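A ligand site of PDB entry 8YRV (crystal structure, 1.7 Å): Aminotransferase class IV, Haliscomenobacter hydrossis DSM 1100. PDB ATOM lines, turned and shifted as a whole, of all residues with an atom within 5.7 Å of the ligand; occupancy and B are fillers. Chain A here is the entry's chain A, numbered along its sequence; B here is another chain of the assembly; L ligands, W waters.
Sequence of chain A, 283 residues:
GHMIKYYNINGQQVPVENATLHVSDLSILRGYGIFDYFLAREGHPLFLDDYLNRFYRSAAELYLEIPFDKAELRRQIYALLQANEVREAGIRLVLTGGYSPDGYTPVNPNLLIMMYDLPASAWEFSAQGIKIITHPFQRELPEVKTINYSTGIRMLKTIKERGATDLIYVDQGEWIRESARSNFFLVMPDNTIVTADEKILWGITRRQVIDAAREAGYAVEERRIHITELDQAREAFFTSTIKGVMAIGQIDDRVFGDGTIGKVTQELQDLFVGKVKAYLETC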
ATOM      1  N   PHE A  35       6.091   1.815  20.961  1.00  0.00           N
ATOM      2  CA  PHE A  35       5.602   2.840  20.022  1.00  0.00           C
ATOM      3  C   PHE A  35       6.801   3.481  19.384  1.00  0.00           C
ATOM      4  O   PHE A  35       7.936   3.257  19.803  1.00  0.00           O
ATOM      5  CB  PHE A  35       4.698   3.844  20.755  1.00  0.00           C
ATOM      6  CG  PHE A  35       5.414   4.960  21.451  1.00  0.00           C
ATOM      7  CD1 PHE A  35       6.137   4.737  22.606  1.00  0.00           C
ATOM      8  CD2 PHE A  35       5.424   6.230  20.902  1.00  0.00           C
ATOM      9  CE1 PHE A  35       6.829   5.781  23.223  1.00  0.00           C
ATOM     10  CE2 PHE A  35       6.046   7.292  21.555  1.00  0.00           C
ATOM     11  CZ  PHE A  35       6.773   7.056  22.703  1.00  0.00           C
ATOM     12  N   ASP A  36       6.519   4.332  18.404  1.00  0.00           N
ATOM     13  CA  ASP A  36       7.540   5.247  17.881  1.00  0.00           C
ATOM     14  C   ASP A  36       6.774   6.491  17.411  1.00  0.00           C
ATOM     15  O   ASP A  36       5.530   6.528  17.411  1.00  0.00           O
ATOM     16  CB  ASP A  36       8.424   4.551  16.833  1.00  0.00           C
ATOM     17  CG  ASP A  36       9.875   4.958  16.973  1.00  0.00           C
ATOM     18  OD1 ASP A  36      10.092   6.192  17.120  1.00  0.00           O
ATOM     19  OD2 ASP A  36      10.713   4.060  17.078  1.00  0.00           O
ATOM     20  N   TYR A  37       7.521   7.537  17.142  1.00  0.00           N
ATOM     21  CA  TYR A  37       6.953   8.859  16.834  1.00  0.00           C
ATOM     22  C   TYR A  37       7.970   9.571  15.965  1.00  0.00           C
ATOM     23  O   TYR A  37       9.142   9.599  16.326  1.00  0.00           O
ATOM     24  CB  TYR A  37       6.641   9.703  18.077  1.00  0.00           C
ATOM     25  CG  TYR A  37       5.756  10.881  17.769  1.00  0.00           C
ATOM     26  CD1 TYR A  37       6.252  12.074  17.290  1.00  0.00           C
ATOM     27  CD2 TYR A  37       4.402  10.795  18.024  1.00  0.00           C
ATOM     28  CE1 TYR A  37       5.400  13.138  16.997  1.00  0.00           C
ATOM     29  CE2 TYR A  37       3.536  11.844  17.752  1.00  0.00           C
ATOM     30  CZ  TYR A  37       4.046  13.020  17.249  1.00  0.00           C
ATOM     31  OH  TYR A  37       3.190  14.046  16.977  1.00  0.00           O
ATOM     32  N   TYR A  51      13.724   5.220  12.209  1.00  0.00           N
ATOM     33  CA  TYR A  51      12.582   5.051  13.129  1.00  0.00           C
ATOM     34  C   TYR A  51      11.954   3.646  12.979  1.00  0.00           C
ATOM     35  O   TYR A  51      11.706   2.985  14.023  1.00  0.00           O
ATOM     36  CB  TYR A  51      11.527   6.110  12.856  1.00  0.00           C
ATOM     37  CG  TYR A  51      11.892   7.468  13.376  1.00  0.00           C
ATOM     38  CD1 TYR A  51      11.771   7.771  14.706  1.00  0.00           C
ATOM     39  CD2 TYR A  51      12.280   8.488  12.514  1.00  0.00           C
ATOM     40  CE1 TYR A  51      12.092   9.035  15.176  1.00  0.00           C
ATOM     41  CE2 TYR A  51      12.591   9.760  12.963  1.00  0.00           C
ATOM     42  CZ  TYR A  51      12.475  10.043  14.302  1.00  0.00           C
ATOM     43  OH  TYR A  51      12.778  11.298  14.762  1.00  0.00           O
ATOM     44  N   ARG A  54      13.957   0.989  14.563  1.00  0.00           N
ATOM     45  CA  ARG A  54      13.812   0.999  16.019  1.00  0.00           C
ATOM     46  C   ARG A  54      12.474   0.369  16.410  1.00  0.00           C
ATOM     47  O   ARG A  54      12.434  -0.390  17.381  1.00  0.00           O
ATOM     48  CB  ARG A  54      13.940   2.417  16.543  1.00  0.00           C
ATOM     49  CG  ARG A  54      13.770   2.480  18.042  1.00  0.00           C
ATOM     50  CD  ARG A  54      14.201   3.846  18.553  1.00  0.00           C
ATOM     51  NE  ARG A  54      13.225   4.859  18.209  1.00  0.00           N
ATOM     52  CZ  ARG A  54      13.332   6.145  18.551  1.00  0.00           C
ATOM     53  NH1 ARG A  54      14.431   6.586  19.152  1.00  0.00           N
ATOM     54  NH2 ARG A  54      12.366   6.982  18.213  1.00  0.00           N
ATOM     55  N   ARG A  92       2.524   8.797  14.969  1.00  0.00           N
ATOM     56  CA  ARG A  92       2.736   7.872  16.107  1.00  0.00           C
ATOM     57  C   ARG A  92       2.439   6.462  15.644  1.00  0.00           C
ATOM     58  O   ARG A  92       1.332   6.225  15.091  1.00  0.00           O
ATOM     59  CB  ARG A  92       1.859   8.272  17.290  1.00  0.00           C
ATOM     60  CG  ARG A  92       2.163   7.433  18.534  1.00  0.00           C
ATOM     61  CD  ARG A  92       1.096   7.677  19.592  1.00  0.00           C
ATOM     62  NE  ARG A  92       0.854   9.085  19.840  1.00  0.00           N
ATOM     63  CZ  ARG A  92       1.490   9.843  20.707  1.00  0.00           C
ATOM     64  NH1 ARG A  92       2.450   9.352  21.490  1.00  0.00           N
ATOM     65  NH2 ARG A  92       1.218  11.128  20.751  1.00  0.00           N
ATOM     66  N   ARG A 139      14.606   4.295  34.083  1.00  0.00           N
ATOM     67  CA  ARG A 139      13.610   3.695  33.141  1.00  0.00           C
ATOM     68  C   ARG A 139      13.781   2.171  33.051  1.00  0.00           C
ATOM     69  O   ARG A 139      14.932   1.702  33.015  1.00  0.00           O
ATOM     70  CB  ARG A 139      13.758   4.301  31.747  1.00  0.00           C
ATOM     71  CG  ARG A 139      13.079   5.656  31.579  1.00  0.00           C
ATOM     72  CD  ARG A 139      13.136   6.155  30.133  1.00  0.00           C
ATOM     73  NE  ARG A 139      12.563   5.191  29.206  1.00  0.00           N
ATOM     74  CZ  ARG A 139      13.258   4.518  28.288  1.00  0.00           C
ATOM     75  NH1 ARG A 139      14.547   4.747  28.146  1.00  0.00           N
ATOM     76  NH2 ARG A 139      12.663   3.615  27.512  1.00  0.00           N
ATOM     77  N   LYS A 145      11.654   1.169  23.172  1.00  0.00           N
ATOM     78  CA  LYS A 145      10.690   2.301  23.227  1.00  0.00           C
ATOM     79  C   LYS A 145       9.335   1.754  23.670  1.00  0.00           C
ATOM     80  O   LYS A 145       8.429   1.665  22.850  1.00  0.00           O
ATOM     81  CB  LYS A 145      10.613   3.037  21.898  1.00  0.00           C
ATOM     82  CG  LYS A 145      10.091   4.463  21.990  1.00  0.00           C
ATOM     83  CD  LYS A 145      10.457   5.253  20.791  1.00  0.00           C
ATOM     84  CE  LYS A 145       9.814   6.619  20.715  1.00  0.00           C
ATOM     85  NZ  LYS A 145      10.769   7.677  21.068  1.00  0.00           N
ATOM     86  N   TYR A 149       5.337   5.253  30.524  1.00  0.00           N
ATOM     87  CA  TYR A 149       5.767   6.638  30.908  1.00  0.00           C
ATOM     88  C   TYR A 149       5.160   7.065  32.263  1.00  0.00           C
ATOM     89  O   TYR A 149       4.985   8.315  32.487  1.00  0.00           O
ATOM     90  CB  TYR A 149       5.446   7.575  29.735  1.00  0.00           C
ATOM     91  CG  TYR A 149       6.419   7.415  28.607  1.00  0.00           C
ATOM     92  CD1 TYR A 149       6.301   6.337  27.740  1.00  0.00           C
ATOM     93  CD2 TYR A 149       7.515   8.248  28.444  1.00  0.00           C
ATOM     94  CE1 TYR A 149       7.198   6.136  26.709  1.00  0.00           C
ATOM     95  CE2 TYR A 149       8.409   8.062  27.382  1.00  0.00           C
ATOM     96  CZ  TYR A 149       8.270   6.979  26.529  1.00  0.00           C
ATOM     97  OH  TYR A 149       9.112   6.720  25.468  1.00  0.00           O
ATOM     98  N   GLU A 178      18.620  10.365  30.763  1.00  0.00           N
ATOM     99  CA  GLU A 178      17.777  11.069  29.776  1.00  0.00           C
ATOM    100  C   GLU A 178      16.577  11.640  30.528  1.00  0.00           C
ATOM    101  O   GLU A 178      16.386  11.303  31.713  1.00  0.00           O
ATOM    102  CB  GLU A 178      17.359  10.137  28.646  1.00  0.00           C
ATOM    103  CG  GLU A 178      16.492   8.981  29.114  1.00  0.00           C
ATOM    104  CD  GLU A 178      16.246   7.925  28.077  1.00  0.00           C
ATOM    105  OE1 GLU A 178      16.216   8.266  26.886  1.00  0.00           O
ATOM    106  OE2 GLU A 178      16.048   6.749  28.519  1.00  0.00           O
ATOM    107  N   SER A 179      15.800  12.496  29.879  1.00  0.00           N
ATOM    108  CA  SER A 179      14.482  12.929  30.378  1.00  0.00           C
ATOM    109  C   SER A 179      13.465  11.819  30.025  1.00  0.00           C
ATOM    110  O   SER A 179      13.864  10.815  29.413  1.00  0.00           O
ATOM    111  CB  SER A 179      14.118  14.255  29.749  1.00  0.00           C
ATOM    112  OG  SER A 179      13.129  14.944  30.479  1.00  0.00           O
ATOM    113  N   ALA A 180      12.200  12.004  30.383  1.00  0.00           N
ATOM    114  CA  ALA A 180      11.142  11.037  30.049  1.00  0.00           C
ATOM    115  C   ALA A 180      10.982  11.034  28.533  1.00  0.00           C
ATOM    116  O   ALA A 180      10.610   9.985  28.009  1.00  0.00           O
ATOM    117  CB  ALA A 180       9.845  11.341  30.765  1.00  0.00           C
ATOM    118  N   ARG A 181      11.280  12.152  27.854  1.00  0.00           N
ATOM    119  CA  ARG A 181      10.958  12.220  26.412  1.00  0.00           C
ATOM    120  C   ARG A 181      12.102  12.793  25.576  1.00  0.00           C
ATOM    121  O   ARG A 181      11.813  13.117  24.398  1.00  0.00           O
ATOM    122  CB  ARG A 181       9.717  13.066  26.227  1.00  0.00           C
ATOM    123  CG  ARG A 181       8.542  12.628  27.103  1.00  0.00           C
ATOM    124  CD  ARG A 181       7.578  13.759  27.158  1.00  0.00           C
ATOM    125  NE  ARG A 181       6.893  13.827  25.912  1.00  0.00           N
ATOM    126  CZ  ARG A 181       5.951  14.705  25.651  1.00  0.00           C
ATOM    127  NH1 ARG A 181       5.659  15.640  26.555  1.00  0.00           N
ATOM    128  NH2 ARG A 181       5.341  14.678  24.466  1.00  0.00           N
ATOM    129  N   SER A 182      13.323  12.853  26.104  1.00  0.00           N
ATOM    130  CA  SER A 182      14.447  13.514  25.400  1.00  0.00           C
ATOM    131  C   SER A 182      15.759  12.869  25.804  1.00  0.00           C
ATOM    132  O   SER A 182      15.890  12.493  26.946  1.00  0.00           O
ATOM    133  CB  SER A 182      14.484  15.000  25.644  1.00  0.00           C
ATOM    134  OG  SER A 182      13.246  15.632  25.289  1.00  0.00           O
ATOM    135  N   ASN A 183      16.718  12.812  24.893  1.00  0.00           N
ATOM    136  CA  ASN A 183      18.086  12.455  25.289  1.00  0.00           C
ATOM    137  C   ASN A 183      18.759  13.718  25.785  1.00  0.00           C
ATOM    138  O   ASN A 183      18.252  14.814  25.530  1.00  0.00           O
ATOM    139  CB  ASN A 183      18.853  11.810  24.130  1.00  0.00           C
ATOM    140  CG  ASN A 183      18.297  10.439  23.833  1.00  0.00           C
ATOM    141  OD1 ASN A 183      17.775  10.222  22.756  1.00  0.00           O
ATOM    142  ND2 ASN A 183      18.521   9.515  24.749  1.00  0.00           N
ATOM    143  N   LEU A 201      17.269   5.354  25.901  1.00  0.00           N
ATOM    144  CA  LEU A 201      16.727   5.104  24.554  1.00  0.00           C
ATOM    145  C   LEU A 201      17.711   5.707  23.561  1.00  0.00           C
ATOM    146  O   LEU A 201      18.155   6.858  23.739  1.00  0.00           O
ATOM    147  CB  LEU A 201      15.362   5.770  24.401  1.00  0.00           C
ATOM    148  CG  LEU A 201      14.635   5.384  23.109  1.00  0.00           C
ATOM    149  CD1 LEU A 201      14.017   4.000  23.262  1.00  0.00           C
ATOM    150  CD2 LEU A 201      13.574   6.429  22.752  1.00  0.00           C
ATOM    151  N   TRP A 202      18.004   4.989  22.489  1.00  0.00           N
ATOM    152  CA  TRP A 202      18.889   5.526  21.441  1.00  0.00           C
ATOM    153  C   TRP A 202      18.031   6.386  20.510  1.00  0.00           C
ATOM    154  O   TRP A 202      17.481   5.892  19.528  1.00  0.00           O
ATOM    155  CB  TRP A 202      19.601   4.395  20.684  1.00  0.00           C
ATOM    156  CG  TRP A 202      20.271   3.395  21.583  1.00  0.00           C
ATOM    157  CD1 TRP A 202      19.734   2.228  22.054  1.00  0.00           C
ATOM    158  CD2 TRP A 202      21.618   3.436  22.062  1.00  0.00           C
ATOM    159  NE1 TRP A 202      20.653   1.554  22.813  1.00  0.00           N
ATOM    160  CE2 TRP A 202      21.823   2.264  22.840  1.00  0.00           C
ATOM    161  CE3 TRP A 202      22.686   4.337  21.911  1.00  0.00           C
ATOM    162  CZ2 TRP A 202      23.040   1.981  23.460  1.00  0.00           C
ATOM    163  CZ3 TRP A 202      23.879   4.047  22.531  1.00  0.00           C
ATOM    164  CH2 TRP A 202      24.048   2.899  23.292  1.00  0.00           C
ATOM    165  N   GLY A 203      17.908   7.659  20.858  1.00  0.00           N
ATOM    166  CA  GLY A 203      17.077   8.609  20.113  1.00  0.00           C
ATOM    167  C   GLY A 203      17.545   8.701  18.661  1.00  0.00           C
ATOM    168  O   GLY A 203      18.778   8.607  18.379  1.00  0.00           O
ATOM    169  N   ILE A 204      16.629   8.902  17.731  1.00  0.00           N
ATOM    170  CA  ILE A 204      17.037   9.188  16.333  1.00  0.00           C
ATOM    171  C   ILE A 204      17.693  10.603  16.328  1.00  0.00           C
ATOM    172  O   ILE A 204      18.725  10.775  15.617  1.00  0.00           O
ATOM    173  CB  ILE A 204      15.823   9.095  15.382  1.00  0.00           C
ATOM    174  CG1 ILE A 204      15.237   7.688  15.259  1.00  0.00           C
ATOM    175  CG2 ILE A 204      16.145   9.712  14.033  1.00  0.00           C
ATOM    176  CD1 ILE A 204      16.049   6.537  15.720  1.00  0.00           C
ATOM    177  N   THR A 205      17.163  11.571  17.086  1.00  0.00           N
ATOM    178  CA  THR A 205      17.717  12.952  17.088  1.00  0.00           C
ATOM    179  C   THR A 205      19.138  12.872  17.646  1.00  0.00           C
ATOM    180  O   THR A 205      20.021  13.482  17.073  1.00  0.00           O
ATOM    181  CB  THR A 205      16.823  13.913  17.875  1.00  0.00           C
ATOM    182  OG1 THR A 205      15.484  13.603  17.512  1.00  0.00           O
ATOM    183  CG2 THR A 205      17.144  15.347  17.559  1.00  0.00           C
ATOM    184  N   ARG A 206      19.285  12.182  18.776  1.00  0.00           N
ATOM    185  CA  ARG A 206      20.600  11.881  19.389  1.00  0.00           C
ATOM    186  C   ARG A 206      21.552  11.384  18.305  1.00  0.00           C
ATOM    187  O   ARG A 206      22.695  11.898  18.247  1.00  0.00           O
ATOM    188  CB  ARG A 206      20.386  10.890  20.521  1.00  0.00           C
ATOM    189  CG  ARG A 206      21.657  10.270  21.086  1.00  0.00           C
ATOM    190  CD  ARG A 206      21.301   9.178  22.098  1.00  0.00           C
ATOM    191  NE  ARG A 206      22.467   8.683  22.817  1.00  0.00           N
ATOM    192  CZ  ARG A 206      23.423   7.943  22.286  1.00  0.00           C
ATOM    193  NH1 ARG A 206      23.320   7.536  21.038  1.00  0.00           N
ATOM    194  NH2 ARG A 206      24.474   7.570  23.009  1.00  0.00           N
ATOM    195  N   THR A 239      17.811  16.432  23.149  1.00  0.00           N
ATOM    196  CA  THR A 239      17.459  16.112  21.758  1.00  0.00           C
ATOM    197  C   THR A 239      16.183  15.287  21.795  1.00  0.00           C
ATOM    198  O   THR A 239      16.070  14.395  22.647  1.00  0.00           O
ATOM    199  CB  THR A 239      18.605  15.381  21.041  1.00  0.00           C
ATOM    200  OG1 THR A 239      18.864  14.123  21.671  1.00  0.00           O
ATOM    201  CG2 THR A 239      19.858  16.209  21.002  1.00  0.00           C
ATOM    202  N   SER A 240      15.289  15.520  20.833  1.00  0.00           N
ATOM    203  CA  SER A 240      14.138  14.616  20.594  1.00  0.00           C
ATOM    204  C   SER A 240      13.551  14.980  19.254  1.00  0.00           C
ATOM    205  O   SER A 240      13.807  16.086  18.698  1.00  0.00           O
ATOM    206  CB  SER A 240      13.079  14.755  21.649  1.00  0.00           C
ATOM    207  OG  SER A 240      12.397  16.010  21.495  1.00  0.00           O
ATOM    208  N   THR A 241      12.709  14.090  18.792  1.00  0.00           N
ATOM    209  CA  THR A 241      11.978  14.227  17.548  1.00  0.00           C
ATOM    210  C   THR A 241      11.255  15.569  17.502  1.00  0.00           C
ATOM    211  O   THR A 241      11.335  16.228  16.461  1.00  0.00           O
ATOM    212  CB  THR A 241      11.007  13.062  17.396  1.00  0.00           C
ATOM    213  OG1 THR A 241      11.826  11.951  17.087  1.00  0.00           O
ATOM    214  CG2 THR A 241      10.007  13.342  16.307  1.00  0.00           C
ATOM    215  N   ILE A 242      10.559  15.947  18.548  1.00  0.00           N
ATOM    216  CA  ILE A 242       9.682  17.154  18.528  1.00  0.00           C
ATOM    217  C   ILE A 242      10.482  18.412  18.935  1.00  0.00           C
ATOM    218  O   ILE A 242      10.132  19.463  18.451  1.00  0.00           O
ATOM    219  CB  ILE A 242       8.421  16.964  19.391  1.00  0.00           C
ATOM    220  CG1 ILE A 242       8.759  16.778  20.876  1.00  0.00           C
ATOM    221  CG2 ILE A 242       7.568  15.822  18.834  1.00  0.00           C
ATOM    222  CD1 ILE A 242       7.747  16.001  21.730  1.00  0.00           C
ATOM    223  N   ARG B  30       0.785   5.650  26.822  1.00  0.00           N
ATOM    224  CA  ARG B  30       1.795   6.013  27.836  1.00  0.00           C
ATOM    225  C   ARG B  30       1.769   5.068  29.049  1.00  0.00           C
ATOM    226  O   ARG B  30       2.450   5.317  30.048  1.00  0.00           O
ATOM    227  CB  ARG B  30       1.605   7.473  28.248  1.00  0.00           C
ATOM    228  CG  ARG B  30       1.846   8.486  27.150  1.00  0.00           C
ATOM    229  CD  ARG B  30       3.267   8.481  26.671  1.00  0.00           C
ATOM    230  NE  ARG B  30       3.439   9.449  25.604  1.00  0.00           N
ATOM    231  CZ  ARG B  30       4.636   9.821  25.135  1.00  0.00           C
ATOM    232  NH1 ARG B  30       5.722   9.247  25.620  1.00  0.00           N
ATOM    233  NH2 ARG B  30       4.739  10.787  24.230  1.00  0.00           N
ATOM    234  N   ASP B 102      -2.336  15.858  24.178  1.00  0.00           N
ATOM    235  CA  ASP B 102      -0.941  15.917  23.689  1.00  0.00           C
ATOM    236  C   ASP B 102      -0.271  14.539  23.834  1.00  0.00           C
ATOM    237  O   ASP B 102       0.930  14.465  23.696  1.00  0.00           O
ATOM    238  CB  ASP B 102      -0.145  17.000  24.444  1.00  0.00           C
ATOM    239  CG  ASP B 102      -0.042  16.709  25.933  1.00  0.00           C
ATOM    240  OD1 ASP B 102      -0.604  15.678  26.399  1.00  0.00           O
ATOM    241  OD2 ASP B 102       0.611  17.506  26.629  1.00  0.00           O
HETATM  242  N1  LIG L   1      14.263   9.086  25.416  1.00  0.00           N
HETATM  243  C1  LIG L   1      12.986   8.746  25.585  1.00  0.00           C
HETATM  244  C2  LIG L   1      12.647   7.933  26.796  1.00  0.00           C
HETATM  245  C3  LIG L   1      11.984   9.177  24.658  1.00  0.00           C
HETATM  246  O1  LIG L   1      10.684   8.827  24.863  1.00  0.00           O
HETATM  247  C4  LIG L   1      12.374   9.949  23.551  1.00  0.00           C
HETATM  248  C5  LIG L   1      11.437  10.473  22.567  1.00  0.00           C
HETATM  249  N2  LIG L   1      10.197  10.260  22.614  1.00  0.00           N
HETATM  250  C6  LIG L   1      13.736  10.281  23.414  1.00  0.00           C
HETATM  251  C7  LIG L   1      14.620   9.816  24.336  1.00  0.00           C
HETATM  252  C8  LIG L   1      14.237  11.002  22.184  1.00  0.00           C
HETATM  253  O2  LIG L   1      14.125  10.035  21.073  1.00  0.00           O
HETATM  254  P1  LIG L   1      13.930  10.580  19.542  1.00  0.00           P
HETATM  255  O3  LIG L   1      15.073  11.587  19.300  1.00  0.00           O
HETATM  256  O4  LIG L   1      12.583  11.331  19.535  1.00  0.00           O
HETATM  257  O5  LIG L   1      14.031   9.343  18.674  1.00  0.00           O
HETATM  258  O6  LIG L   1       9.509  11.098  21.711  1.00  0.00           O
HETATM  259  C9  LIG L   1       8.222  10.499  21.448  1.00  0.00           C
HETATM  260  C10 LIG L   1       7.210  11.539  21.050  1.00  0.00           C
HETATM  261  C11 LIG L   1       6.671  12.417  22.167  1.00  0.00           C
HETATM  262  O7  LIG L   1       7.249  12.421  23.253  1.00  0.00           O
HETATM  263  O8  LIG L   1       5.651  13.118  21.942  1.00  0.00           O
HETATM  264  O   HOH W   1       9.436  13.587  23.062  1.00  0.00           O
HETATM  265  O   HOH W   2      10.360   9.669  18.908  1.00  0.00           O
HETATM  266  O   HOH W   3      17.285  11.971  20.721  1.00  0.00           O
HETATM  267  O   HOH W   4       2.821  12.438  22.844  1.00  0.00           O
HETATM  268  O   HOH W   5       3.949  14.407  20.802  1.00  0.00           O
HETATM  269  O   HOH W   6       9.989  13.636  20.561  1.00  0.00           O
HETATM  270  O   HOH W   7       8.311  10.244  24.952  1.00  0.00           O
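The guanidinium group (NH1) of Arg 54 is in salt-bridge range of an oxygen (O5) of the ligand (2.8 Å).
N of Thr 241 lies within hydrogen-bond range of O4 of the ligand.
The side-chain hydroxyl (OG1) of Thr 241 sits at hydrogen-bond distance from an oxygen (O4) of the ligand (2.6 Å).
An oxygen (O8) of the ligand lies within salt-bridge range of the guanidinium group of Arg 181, 3.0 Å away.
The backbone NH of Ile 204 is in hydrogen-bond range of an oxygen (O5) of the ligand, at 2.8 Å.
OG1 of Thr 205 is in hydrogen-bond range of O3 of the ligand (2.7 Å).
O1 of the ligand sits at hydrogen-bond distance from OH of Tyr 149 (2.7 Å).
The backbone carbonyl oxygen (O) of Ala 180 lies close to an oxygen (O1) of the ligand, at 3.4 Å.
A nitrogen (N2) of the ligand lies within hydrogen-bond range of the side-chain amino group of Lys 145.
The side-chain carboxylate (OE1) of Glu 178 sits at hydrogen-bond distance from a nitrogen (N1) of the ligand (2.6 Å).
NH2 of Arg 30 of chain B lies within salt-bridge range of O7 of the ligand (3.2 Å).
N of Thr 205 is in hydrogen-bond range of O3 of the ligand, at 3.0 Å.
Residues that only touch the ligand: Gly 203 (3.4 Å), Ser 240 (3.4 Å), Tyr 37 (3.5 Å), Asn 183 (3.6 Å), Ile 242 (3.6 Å), Ser 182 (3.6 Å), Leu 201 (3.6 Å), Arg 139 (3.7 Å), Phe 35 (3.9 Å) and Thr 239 (3.9 Å).
Hydrophobic or aromatic side chains that line the ligand: Phe 35, Tyr 37, Tyr 149, Leu 201, Ile 204 and Ile 242.
Of the 27 residues printed, 20 come within 4 Å of the ligand.
The side-chain carboxylate (OE1) of Glu 178 lies within hydrogen-bond range of the side-chain amide nitrogen (ND2) of Asn 183.
The side-chain hydroxyl (OG1) of Thr 241 lies within hydrogen-bond range of the side-chain hydroxyl (OH) of Tyr 51.
N of Thr 241 lies within hydrogen-bond range of OG1 of Thr 205 (3.1 Å).
The guanidinium group of Arg 54 is in salt-bridge range of the side-chain carboxylate of Asp 36, at 2.6 Å.
The guanidinium group (NH1) of Arg 54 lies within hydrogen-bond range of the backbone carbonyl oxygen (O) of Trp 202.
The side-chain hydroxyl (OG1) of Thr 205 sits close to the backbone carbonyl oxygen (O) of Ser 240 (3.2 Å).
OE2 of Glu 178 is in salt-bridge range of NH1 of Arg 139.
N of Asn 183 is in hydrogen-bond range of O of Thr 239 (2.8 Å).
Water W1 lies within hydrogen-bond range of an oxygen (O7) of the ligand and the backbone carbonyl oxygen (O) of Arg 181.
Water W3 lies within hydrogen-bond range of O3 of the ligand (2.7 Å), OD1 of Asn 183 (2.7 Å), N of Arg 206 (2.8 Å) and OG1 of Thr 239 (2.8 Å).
Water W7 bridges O1 of the ligand and NH1 of Arg 30 of chain B.
Water W6 lies within hydrogen-bond range of O6 of the ligand (2.8 Å), N of Ile 242 (3.1 Å) and N of Thr 241 (3.3 Å).
Water W2 lies within hydrogen-bond range of O4 of the ligand (2.8 Å), O of Tyr 37 (2.9 Å), NZ of Lys 145 (3.0 Å), OG1 of Thr 241 (3.3 Å) and NH2 of Arg 54 (3.4 Å).
Water W4 lies within hydrogen-bond range of NH2 of Arg 30 of chain B (2.9 Å), O of Asp 102 of chain B (2.9 Å), NH2 of Arg 92 (2.9 Å) and O8 of the ligand (3.0 Å).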
